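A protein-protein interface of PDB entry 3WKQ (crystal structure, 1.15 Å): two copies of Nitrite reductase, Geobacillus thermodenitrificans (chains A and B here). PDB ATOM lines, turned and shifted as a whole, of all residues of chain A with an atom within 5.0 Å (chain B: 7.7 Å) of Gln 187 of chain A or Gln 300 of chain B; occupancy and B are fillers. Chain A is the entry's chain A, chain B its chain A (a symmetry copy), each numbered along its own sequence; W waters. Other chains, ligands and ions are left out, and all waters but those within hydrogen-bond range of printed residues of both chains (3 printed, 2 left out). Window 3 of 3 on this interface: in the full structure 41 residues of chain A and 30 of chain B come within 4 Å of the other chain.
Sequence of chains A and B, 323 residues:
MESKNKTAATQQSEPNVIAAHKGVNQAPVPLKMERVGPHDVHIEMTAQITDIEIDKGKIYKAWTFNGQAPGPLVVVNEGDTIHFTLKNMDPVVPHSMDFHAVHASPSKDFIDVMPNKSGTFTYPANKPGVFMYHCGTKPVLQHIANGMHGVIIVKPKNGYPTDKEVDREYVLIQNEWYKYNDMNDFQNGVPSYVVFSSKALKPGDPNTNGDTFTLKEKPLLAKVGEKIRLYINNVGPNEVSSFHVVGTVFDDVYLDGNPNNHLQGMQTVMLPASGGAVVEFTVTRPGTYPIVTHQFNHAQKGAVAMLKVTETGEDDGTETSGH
OD1 of Asn 188 of chain A lies within hydrogen-bond range of NZ of Lys 301 of chain B (2.8 Å).
The backbone carbonyl oxygen (O) of Gln 187 of chain A is in hydrogen-bond range of the side-chain amino group (NZ) of Lys 301 of chain B (3.0 Å).
The backbone NH (N) of Val 194 of chain B is in hydrogen-bond range of the backbone carbonyl oxygen (O) of Lys 301 of chain B (3.1 Å).
OE1 of Gln 187 of chain A lies close to O of Met 183 of chain A, 3.0 Å away.
The side-chain amide oxygen (OD1) of Asn 184 of chain A sits at hydrogen-bond distance from the side-chain amide nitrogen (ND2) of Asn 188 of chain A (3.0 Å).
O of Pro 191 of chain B lies within hydrogen-bond range of NZ of Lys 301 of chain B.
Among the printed residues, pairs that only touch across the chains: Pro 139 of chain A with Gln 300 of chain B, Val 140 of chain A with Phe 296 of chain B, Leu 141 of chain A with Phe 296 of chain B, Leu 141 of chain A with Asn 297 of chain B, Leu 141 of chain A with Gln 300 of chain B, Met 183 of chain A with Gln 300 of chain B, Phe 186 of chain A with Asn 297 of chain B, Gln 187 of chain A with Asn 297 of chain B, Gln 187 of chain A with Gln 300 of chain B and Asn 188 of chain A with Val 190 of chain B.
Gln 187 of chain A touches just these residues of chain B: Asn 297 (3.4 Å), Gln 300 (3.6 Å) and Lys 301 (3.0 Å).
Of the printed residues of chain A, Gln 300 of chain B touches Pro 139 (3.6 Å), Leu 141 (3.7 Å), Met 183 (3.7 Å) and Gln 187 (3.6 Å).
Of the printed residues of chain A, Phe 296 of chain B touches Val 140 (3.6 Å) and Leu 141 (3.9 Å).
Of the printed residues of chain B, Met 183 of chain A touches Gln 300 (3.7 Å).
Of the printed residues of chain A, Asn 297 of chain B touches Leu 141 (3.9 Å), Phe 186 (3.5 Å) and Gln 187 (3.4 Å).
Gly 302 of chain B touches none of the printed residues of chain A.
The nearest residue of chain B that does not touch Gln 187 of chain A is Val 190 of chain B (5.3 Å).
Of the 18 printed residues of chain B, 5 touch a printed residue of chain A.
Hydrophobic or aromatic side chains of chain A that line the printed part of chain B: Pro 139, Val 140, Leu 141 and Met 183.
Along chain A the printed residues that touch a printed residue of chain B span positions 139 to 188.
Among the printed residues, 12 pairs touch across the chains.
No position is printed for both chains.
Water W1 lies within hydrogen-bond range of the backbone carbonyl oxygen (O) of Gly 189 of chain A, the backbone carbonyl oxygen (O) of Phe 186 of chain A and the side-chain amide nitrogen (ND2) of Asn 297 of chain B.
Water W2 lies within hydrogen-bond range of OE1 of Gln 300 of chain B (2.8 Å), N of Leu 141 of chain A (2.9 Å) and N of Val 140 of chain A (3.4 Å).
Water W3 lies within hydrogen-bond range of NE2 of Gln 187 of chain A (2.8 Å) and NE2 of Gln 300 of chain B (3.0 Å).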
ATOM      1  N   PRO A 139      29.634 -13.194  -3.329  1.00  0.00           N
ATOM      2  CA  PRO A 139      28.620 -12.214  -2.867  1.00  0.00           C
ATOM      3  C   PRO A 139      27.550 -11.981  -3.925  1.00  0.00           C
ATOM      4  O   PRO A 139      27.888 -11.634  -5.083  1.00  0.00           O
ATOM      5  CB  PRO A 139      29.426 -10.887  -2.682  1.00  0.00           C
ATOM      6  CG  PRO A 139      30.835 -11.256  -2.970  1.00  0.00           C
ATOM      7  CD  PRO A 139      30.860 -12.516  -3.706  1.00  0.00           C
ATOM      8  N   VAL A 140      26.300 -12.160  -3.566  1.00  0.00           N
ATOM      9  CA  VAL A 140      25.254 -12.090  -4.572  1.00  0.00           C
ATOM     10  C   VAL A 140      25.186 -10.737  -5.206  1.00  0.00           C
ATOM     11  O   VAL A 140      24.962 -10.605  -6.412  1.00  0.00           O
ATOM     12  CB  VAL A 140      23.899 -12.506  -3.933  1.00  0.00           C
ATOM     13  CG1 VAL A 140      22.732 -12.308  -4.893  1.00  0.00           C
ATOM     14  CG2 VAL A 140      24.014 -14.007  -3.519  1.00  0.00           C
ATOM     15  N   LEU A 141      25.422  -9.649  -4.428  1.00  0.00           N
ATOM     16  CA  LEU A 141      25.469  -8.339  -5.033  1.00  0.00           C
ATOM     17  C   LEU A 141      26.413  -8.273  -6.204  1.00  0.00           C
ATOM     18  O   LEU A 141      26.114  -7.629  -7.209  1.00  0.00           O
ATOM     19  CB  LEU A 141      25.883  -7.314  -3.977  1.00  0.00           C
ATOM     20  CG  LEU A 141      26.147  -5.880  -4.498  1.00  0.00           C
ATOM     21  CD1 LEU A 141      24.961  -5.207  -5.126  1.00  0.00           C
ATOM     22  CD2 LEU A 141      26.683  -5.052  -3.326  1.00  0.00           C
ATOM     23  N   MET A 183      33.133  -3.537  -5.985  1.00  0.00           N
ATOM     24  CA  MET A 183      32.244  -3.798  -4.862  1.00  0.00           C
ATOM     25  C   MET A 183      31.997  -2.590  -4.008  1.00  0.00           C
ATOM     26  O   MET A 183      30.914  -2.466  -3.408  1.00  0.00           O
ATOM     27  CB  MET A 183      32.741  -5.000  -4.022  1.00  0.00           C
ATOM     28  CG  MET A 183      32.286  -6.397  -4.654  1.00  0.00           C
ATOM     29  SD  MET A 183      30.598  -6.680  -4.339  1.00  0.00           S
ATOM     30  CE  MET A 183      30.557  -7.195  -2.619  1.00  0.00           C
ATOM     31  N   ASN A 184      32.953  -1.675  -3.893  1.00  0.00           N
ATOM     32  CA  ASN A 184      32.691  -0.460  -3.131  1.00  0.00           C
ATOM     33  C   ASN A 184      31.602   0.327  -3.789  1.00  0.00           C
ATOM     34  O   ASN A 184      30.663   0.803  -3.153  1.00  0.00           O
ATOM     35  CB  ASN A 184      33.992   0.347  -3.032  1.00  0.00           C
ATOM     36  CG  ASN A 184      33.721   1.576  -2.220  1.00  0.00           C
ATOM     37  OD1 ASN A 184      33.214   1.508  -1.086  1.00  0.00           O
ATOM     38  ND2 ASN A 184      33.818   2.717  -2.909  1.00  0.00           N
ATOM     39  N   ASP A 185      31.680   0.502  -5.107  1.00  0.00           N
ATOM     40  CA  ASP A 185      30.639   1.218  -5.852  1.00  0.00           C
ATOM     41  C   ASP A 185      29.344   0.473  -5.786  1.00  0.00           C
ATOM     42  O   ASP A 185      28.275   1.080  -5.630  1.00  0.00           O
ATOM     43  CB  ASP A 185      31.082   1.427  -7.275  1.00  0.00           C
ATOM     44  CG  ASP A 185      30.277   2.478  -8.021  1.00  0.00           C
ATOM     45  OD1 ASP A 185      30.219   3.607  -7.477  1.00  0.00           O
ATOM     46  OD2 ASP A 185      29.769   2.191  -9.115  1.00  0.00           O
ATOM     47  N   PHE A 186      29.340  -0.826  -5.927  1.00  0.00           N
ATOM     48  CA  PHE A 186      28.105  -1.618  -5.858  1.00  0.00           C
ATOM     49  C   PHE A 186      27.380  -1.399  -4.573  1.00  0.00           C
ATOM     50  O   PHE A 186      26.141  -1.355  -4.551  1.00  0.00           O
ATOM     51  CB  PHE A 186      28.380  -3.125  -6.006  1.00  0.00           C
ATOM     52  CG  PHE A 186      28.942  -3.576  -7.323  1.00  0.00           C
ATOM     53  CD1 PHE A 186      29.051  -2.804  -8.462  1.00  0.00           C
ATOM     54  CD2 PHE A 186      29.396  -4.944  -7.395  1.00  0.00           C
ATOM     55  CE1 PHE A 186      29.541  -3.319  -9.652  1.00  0.00           C
ATOM     56  CE2 PHE A 186      29.899  -5.462  -8.595  1.00  0.00           C
ATOM     57  CZ  PHE A 186      29.949  -4.651  -9.753  1.00  0.00           C
ATOM     58  N   GLN A 187      28.130  -1.281  -3.474  1.00  0.00           N
ATOM     59  CA  GLN A 187      27.474  -1.117  -2.164  1.00  0.00           C
ATOM     60  C   GLN A 187      27.149   0.296  -1.761  1.00  0.00           C
ATOM     61  O   GLN A 187      26.234   0.484  -0.979  1.00  0.00           O
ATOM     62  CB  GLN A 187      28.494  -1.683  -1.058  1.00  0.00           C
ATOM     63  CG  GLN A 187      28.697  -3.079  -0.994  1.00  0.00           C
ATOM     64  CD  GLN A 187      29.851  -3.307  -0.043  1.00  0.00           C
ATOM     65  OE1 GLN A 187      30.893  -3.539  -0.597  1.00  0.00           O
ATOM     66  NE2 GLN A 187      29.668  -3.310   1.189  1.00  0.00           N
ATOM     67  N   ASN A 188      27.964   1.275  -2.260  1.00  0.00           N
ATOM     68  CA  ASN A 188      27.924   2.613  -1.700  1.00  0.00           C
ATOM     69  C   ASN A 188      27.693   3.689  -2.776  1.00  0.00           C
ATOM     70  O   ASN A 188      27.522   4.860  -2.320  1.00  0.00           O
ATOM     71  CB  ASN A 188      29.229   2.879  -0.941  1.00  0.00           C
ATOM     72  CG  ASN A 188      29.399   1.996   0.227  1.00  0.00           C
ATOM     73  OD1 ASN A 188      28.510   1.846   1.040  1.00  0.00           O
ATOM     74  ND2 ASN A 188      30.564   1.344   0.340  1.00  0.00           N
ATOM     75  N   GLY A 189      27.762   3.389  -4.045  1.00  0.00           N
ATOM     76  CA  GLY A 189      27.685   4.425  -5.089  1.00  0.00           C
ATOM     77  C   GLY A 189      26.342   4.490  -5.725  1.00  0.00           C
ATOM     78  O   GLY A 189      25.596   3.511  -5.824  1.00  0.00           O
ATOM     79  N   VAL B 190      25.042   7.208   2.884  1.00  0.00           N
ATOM     80  CA  VAL B 190      24.515   5.869   2.781  1.00  0.00           C
ATOM     81  C   VAL B 190      24.648   5.161   4.136  1.00  0.00           C
ATOM     82  O   VAL B 190      25.574   5.425   4.915  1.00  0.00           O
ATOM     83  CB  VAL B 190      25.255   5.031   1.686  1.00  0.00           C
ATOM     84  CG1 VAL B 190      24.989   5.641   0.310  1.00  0.00           C
ATOM     85  CG2 VAL B 190      26.751   4.822   1.989  1.00  0.00           C
ATOM     86  N   PRO B 191      23.789   4.177   4.408  1.00  0.00           N
ATOM     87  CA  PRO B 191      23.950   3.430   5.670  1.00  0.00           C
ATOM     88  C   PRO B 191      25.250   2.635   5.642  1.00  0.00           C
ATOM     89  O   PRO B 191      25.688   2.119   4.636  1.00  0.00           O
ATOM     90  CB  PRO B 191      22.709   2.501   5.657  1.00  0.00           C
ATOM     91  CG  PRO B 191      22.309   2.407   4.258  1.00  0.00           C
ATOM     92  CD  PRO B 191      22.614   3.737   3.623  1.00  0.00           C
ATOM     93  N   SER B 192      25.885   2.543   6.838  1.00  0.00           N
ATOM     94  CA  SER B 192      27.040   1.685   7.011  1.00  0.00           C
ATOM     95  C   SER B 192      26.656   0.235   7.081  1.00  0.00           C
ATOM     96  O   SER B 192      27.375  -0.634   6.622  1.00  0.00           O
ATOM     97  CB  SER B 192      27.804   2.124   8.210  1.00  0.00           C
ATOM     98  OG  SER B 192      28.453   3.393   8.036  1.00  0.00           O
ATOM     99  N   TYR B 193      25.526  -0.026   7.766  1.00  0.00           N
ATOM    100  CA  TYR B 193      25.020  -1.365   7.934  1.00  0.00           C
ATOM    101  C   TYR B 193      23.503  -1.331   7.749  1.00  0.00           C
ATOM    102  O   TYR B 193      22.890  -0.304   8.104  1.00  0.00           O
ATOM    103  CB  TYR B 193      25.299  -1.936   9.353  1.00  0.00           C
ATOM    104  CG  TYR B 193      26.769  -1.798   9.742  1.00  0.00           C
ATOM    105  CD1 TYR B 193      27.681  -2.733   9.280  1.00  0.00           C
ATOM    106  CD2 TYR B 193      27.195  -0.700  10.477  1.00  0.00           C
ATOM    107  CE1 TYR B 193      29.098  -2.507   9.667  1.00  0.00           C
ATOM    108  CE2 TYR B 193      28.554  -0.523  10.792  1.00  0.00           C
ATOM    109  CZ  TYR B 193      29.437  -1.373  10.387  1.00  0.00           C
ATOM    110  OH  TYR B 193      30.770  -1.143  10.778  1.00  0.00           O
ATOM    111  N   VAL B 194      22.949  -2.415   7.255  1.00  0.00           N
ATOM    112  CA  VAL B 194      21.500  -2.580   7.226  1.00  0.00           C
ATOM    113  C   VAL B 194      21.289  -3.973   7.774  1.00  0.00           C
ATOM    114  O   VAL B 194      22.053  -4.900   7.422  1.00  0.00           O
ATOM    115  CB  VAL B 194      20.898  -2.403   5.800  1.00  0.00           C
ATOM    116  CG1 VAL B 194      19.392  -2.502   5.883  1.00  0.00           C
ATOM    117  CG2 VAL B 194      21.340  -1.103   5.189  1.00  0.00           C
ATOM    118  N   THR B 212      24.620  -7.511  12.042  1.00  0.00           N
ATOM    119  CA  THR B 212      24.863  -8.092  10.736  1.00  0.00           C
ATOM    120  C   THR B 212      24.990  -9.610  10.746  1.00  0.00           C
ATOM    121  O   THR B 212      25.209 -10.197   9.677  1.00  0.00           O
ATOM    122  CB  THR B 212      26.145  -7.536  10.143  1.00  0.00           C
ATOM    123  OG1 THR B 212      27.179  -7.947  11.043  1.00  0.00           O
ATOM    124  CG2 THR B 212      26.138  -6.028   9.999  1.00  0.00           C
ATOM    125  N   LYS B 216      22.307 -14.977  10.933  1.00  0.00           N
ATOM    126  CA  LYS B 216      23.037 -15.895  10.078  1.00  0.00           C
ATOM    127  C   LYS B 216      23.604 -17.024  10.882  1.00  0.00           C
ATOM    128  O   LYS B 216      23.523 -18.222  10.479  1.00  0.00           O
ATOM    129  CB  LYS B 216      24.196 -15.165   9.390  1.00  0.00           C
ATOM    130  CG  LYS B 216      23.783 -14.093   8.454  1.00  0.00           C
ATOM    131  CD  LYS B 216      25.026 -13.343   7.937  1.00  0.00           C
ATOM    132  CE  LYS B 216      24.793 -12.305   6.881  1.00  0.00           C
ATOM    133  NZ  LYS B 216      23.949 -11.145   7.345  1.00  0.00           N
ATOM    134  N   THR B 293      16.565  -8.117   2.270  1.00  0.00           N
ATOM    135  CA  THR B 293      16.072  -7.063   1.397  1.00  0.00           C
ATOM    136  C   THR B 293      16.780  -7.231   0.053  1.00  0.00           C
ATOM    137  O   THR B 293      18.002  -7.416   0.001  1.00  0.00           O
ATOM    138  CB  THR B 293      16.250  -5.661   1.994  1.00  0.00           C
ATOM    139  OG1 THR B 293      15.778  -4.738   0.971  1.00  0.00           O
ATOM    140  CG2 THR B 293      17.693  -5.362   2.334  1.00  0.00           C
ATOM    141  N   GLN B 295      17.244  -5.140  -2.204  1.00  0.00           N
ATOM    142  CA  GLN B 295      18.172  -4.016  -2.539  1.00  0.00           C
ATOM    143  C   GLN B 295      19.528  -4.516  -2.055  1.00  0.00           C
ATOM    144  O   GLN B 295      19.855  -4.480  -0.897  1.00  0.00           O
ATOM    145  CB  GLN B 295      17.685  -2.760  -1.843  1.00  0.00           C
ATOM    146  CG  GLN B 295      16.369  -2.275  -2.449  1.00  0.00           C
ATOM    147  CD  GLN B 295      15.536  -1.420  -1.456  1.00  0.00           C
ATOM    148  OE1 GLN B 295      14.423  -1.740  -1.162  1.00  0.00           O
ATOM    149  NE2 GLN B 295      16.151  -0.342  -0.931  1.00  0.00           N
ATOM    150  N   PHE B 296      20.262  -5.062  -3.024  1.00  0.00           N
ATOM    151  CA  PHE B 296      21.384  -5.897  -2.609  1.00  0.00           C
ATOM    152  C   PHE B 296      22.567  -5.165  -2.023  1.00  0.00           C
ATOM    153  O   PHE B 296      23.362  -5.777  -1.302  1.00  0.00           O
ATOM    154  CB  PHE B 296      21.791  -6.924  -3.705  1.00  0.00           C
ATOM    155  CG  PHE B 296      21.316  -8.318  -3.352  1.00  0.00           C
ATOM    156  CD1 PHE B 296      22.098  -9.100  -2.495  1.00  0.00           C
ATOM    157  CD2 PHE B 296      20.074  -8.807  -3.756  1.00  0.00           C
ATOM    158  CE1 PHE B 296      21.680 -10.346  -2.060  1.00  0.00           C
ATOM    159  CE2 PHE B 296      19.658 -10.068  -3.309  1.00  0.00           C
ATOM    160  CZ  PHE B 296      20.445 -10.821  -2.457  1.00  0.00           C
ATOM    161  N   ASN B 297      22.674  -3.866  -2.243  1.00  0.00           N
ATOM    162  CA  ASN B 297      23.676  -3.107  -1.512  1.00  0.00           C
ATOM    163  C   ASN B 297      23.423  -3.191   0.002  1.00  0.00           C
ATOM    164  O   ASN B 297      24.350  -3.338   0.774  1.00  0.00           O
ATOM    165  CB  ASN B 297      23.786  -1.661  -2.013  1.00  0.00           C
ATOM    166  CG  ASN B 297      22.468  -0.894  -2.081  1.00  0.00           C
ATOM    167  OD1 ASN B 297      21.390  -1.412  -1.872  1.00  0.00           O
ATOM    168  ND2 ASN B 297      22.581   0.373  -2.521  1.00  0.00           N
ATOM    169  N   HIS B 298      22.148  -3.144   0.405  1.00  0.00           N
ATOM    170  CA  HIS B 298      21.768  -3.265   1.794  1.00  0.00           C
ATOM    171  C   HIS B 298      21.975  -4.670   2.308  1.00  0.00           C
ATOM    172  O   HIS B 298      22.449  -4.899   3.429  1.00  0.00           O
ATOM    173  CB  HIS B 298      20.324  -2.826   1.979  1.00  0.00           C
ATOM    174  CG  HIS B 298      20.099  -1.429   1.642  1.00  0.00           C
ATOM    175  ND1 HIS B 298      18.812  -0.936   1.469  1.00  0.00           N
ATOM    176  CD2 HIS B 298      20.975  -0.384   1.381  1.00  0.00           C
ATOM    177  CE1 HIS B 298      18.940   0.335   1.138  1.00  0.00           C
ATOM    178  NE2 HIS B 298      20.204   0.731   1.066  1.00  0.00           N
ATOM    179  N   ALA B 299      21.624  -5.696   1.486  1.00  0.00           N
ATOM    180  CA  ALA B 299      21.874  -7.061   1.857  1.00  0.00           C
ATOM    181  C   ALA B 299      23.369  -7.282   2.114  1.00  0.00           C
ATOM    182  O   ALA B 299      23.779  -7.920   3.096  1.00  0.00           O
ATOM    183  CB  ALA B 299      21.368  -8.018   0.771  1.00  0.00           C
ATOM    184  N   GLN B 300      24.229  -6.765   1.211  1.00  0.00           N
ATOM    185  CA  GLN B 300      25.645  -6.933   1.366  1.00  0.00           C
ATOM    186  C   GLN B 300      26.175  -6.267   2.634  1.00  0.00           C
ATOM    187  O   GLN B 300      27.143  -6.734   3.229  1.00  0.00           O
ATOM    188  CB  GLN B 300      26.336  -6.360   0.141  1.00  0.00           C
ATOM    189  CG  GLN B 300      27.876  -6.431   0.186  1.00  0.00           C
ATOM    190  CD  GLN B 300      28.422  -7.843   0.273  1.00  0.00           C
ATOM    191  OE1 GLN B 300      27.821  -8.807  -0.229  1.00  0.00           O
ATOM    192  NE2 GLN B 300      29.619  -7.972   0.854  1.00  0.00           N
ATOM    193  N   LYS B 301      25.531  -5.187   3.070  1.00  0.00           N
ATOM    194  CA  LYS B 301      25.884  -4.447   4.289  1.00  0.00           C
ATOM    195  C   LYS B 301      25.196  -4.999   5.519  1.00  0.00           C
ATOM    196  O   LYS B 301      25.226  -4.323   6.561  1.00  0.00           O
ATOM    197  CB  LYS B 301      25.680  -2.956   4.037  1.00  0.00           C
ATOM    198  CG  LYS B 301      26.683  -2.388   3.052  1.00  0.00           C
ATOM    199  CD  LYS B 301      26.832  -0.927   2.874  1.00  0.00           C
ATOM    200  CE  LYS B 301      25.627  -0.353   2.218  1.00  0.00           C
ATOM    201  NZ  LYS B 301      25.898   1.185   1.956  1.00  0.00           N
ATOM    202  N   GLY B 302      24.645  -6.205   5.433  1.00  0.00           N
ATOM    203  CA  GLY B 302      24.207  -6.921   6.635  1.00  0.00           C
ATOM    204  C   GLY B 302      22.860  -7.507   6.571  1.00  0.00           C
ATOM    205  O   GLY B 302      22.529  -8.360   7.435  1.00  0.00           O
ATOM    206  N   ALA B 303      21.983  -7.104   5.645  1.00  0.00           N
ATOM    207  CA  ALA B 303      20.550  -7.367   5.741  1.00  0.00           C
ATOM    208  C   ALA B 303      20.205  -8.690   5.058  1.00  0.00           C
ATOM    209  O   ALA B 303      19.477  -8.779   4.099  1.00  0.00           O
ATOM    210  CB  ALA B 303      19.749  -6.228   5.170  1.00  0.00           C
ATOM    211  N   VAL B 304      20.721  -9.759   5.707  1.00  0.00           N
ATOM    212  CA  VAL B 304      20.413 -11.137   5.382  1.00  0.00           C
ATOM    213  C   VAL B 304      20.246 -11.910   6.675  1.00  0.00           C
ATOM    214  O   VAL B 304      21.182 -11.901   7.518  1.00  0.00           O
ATOM    215  CB  VAL B 304      21.497 -11.810   4.505  1.00  0.00           C
ATOM    216  CG1 VAL B 304      21.169 -13.256   4.219  1.00  0.00           C
ATOM    217  CG2 VAL B 304      21.747 -11.028   3.236  1.00  0.00           C
HETATM  218  O   HOH W   1      25.003   1.266  -4.342  1.00  0.00           O
HETATM  219  O   HOH W   2      25.484  -9.607  -1.548  1.00  0.00           O
HETATM  220  O   HOH W   3      30.751  -5.618   2.373  1.00  0.00           O
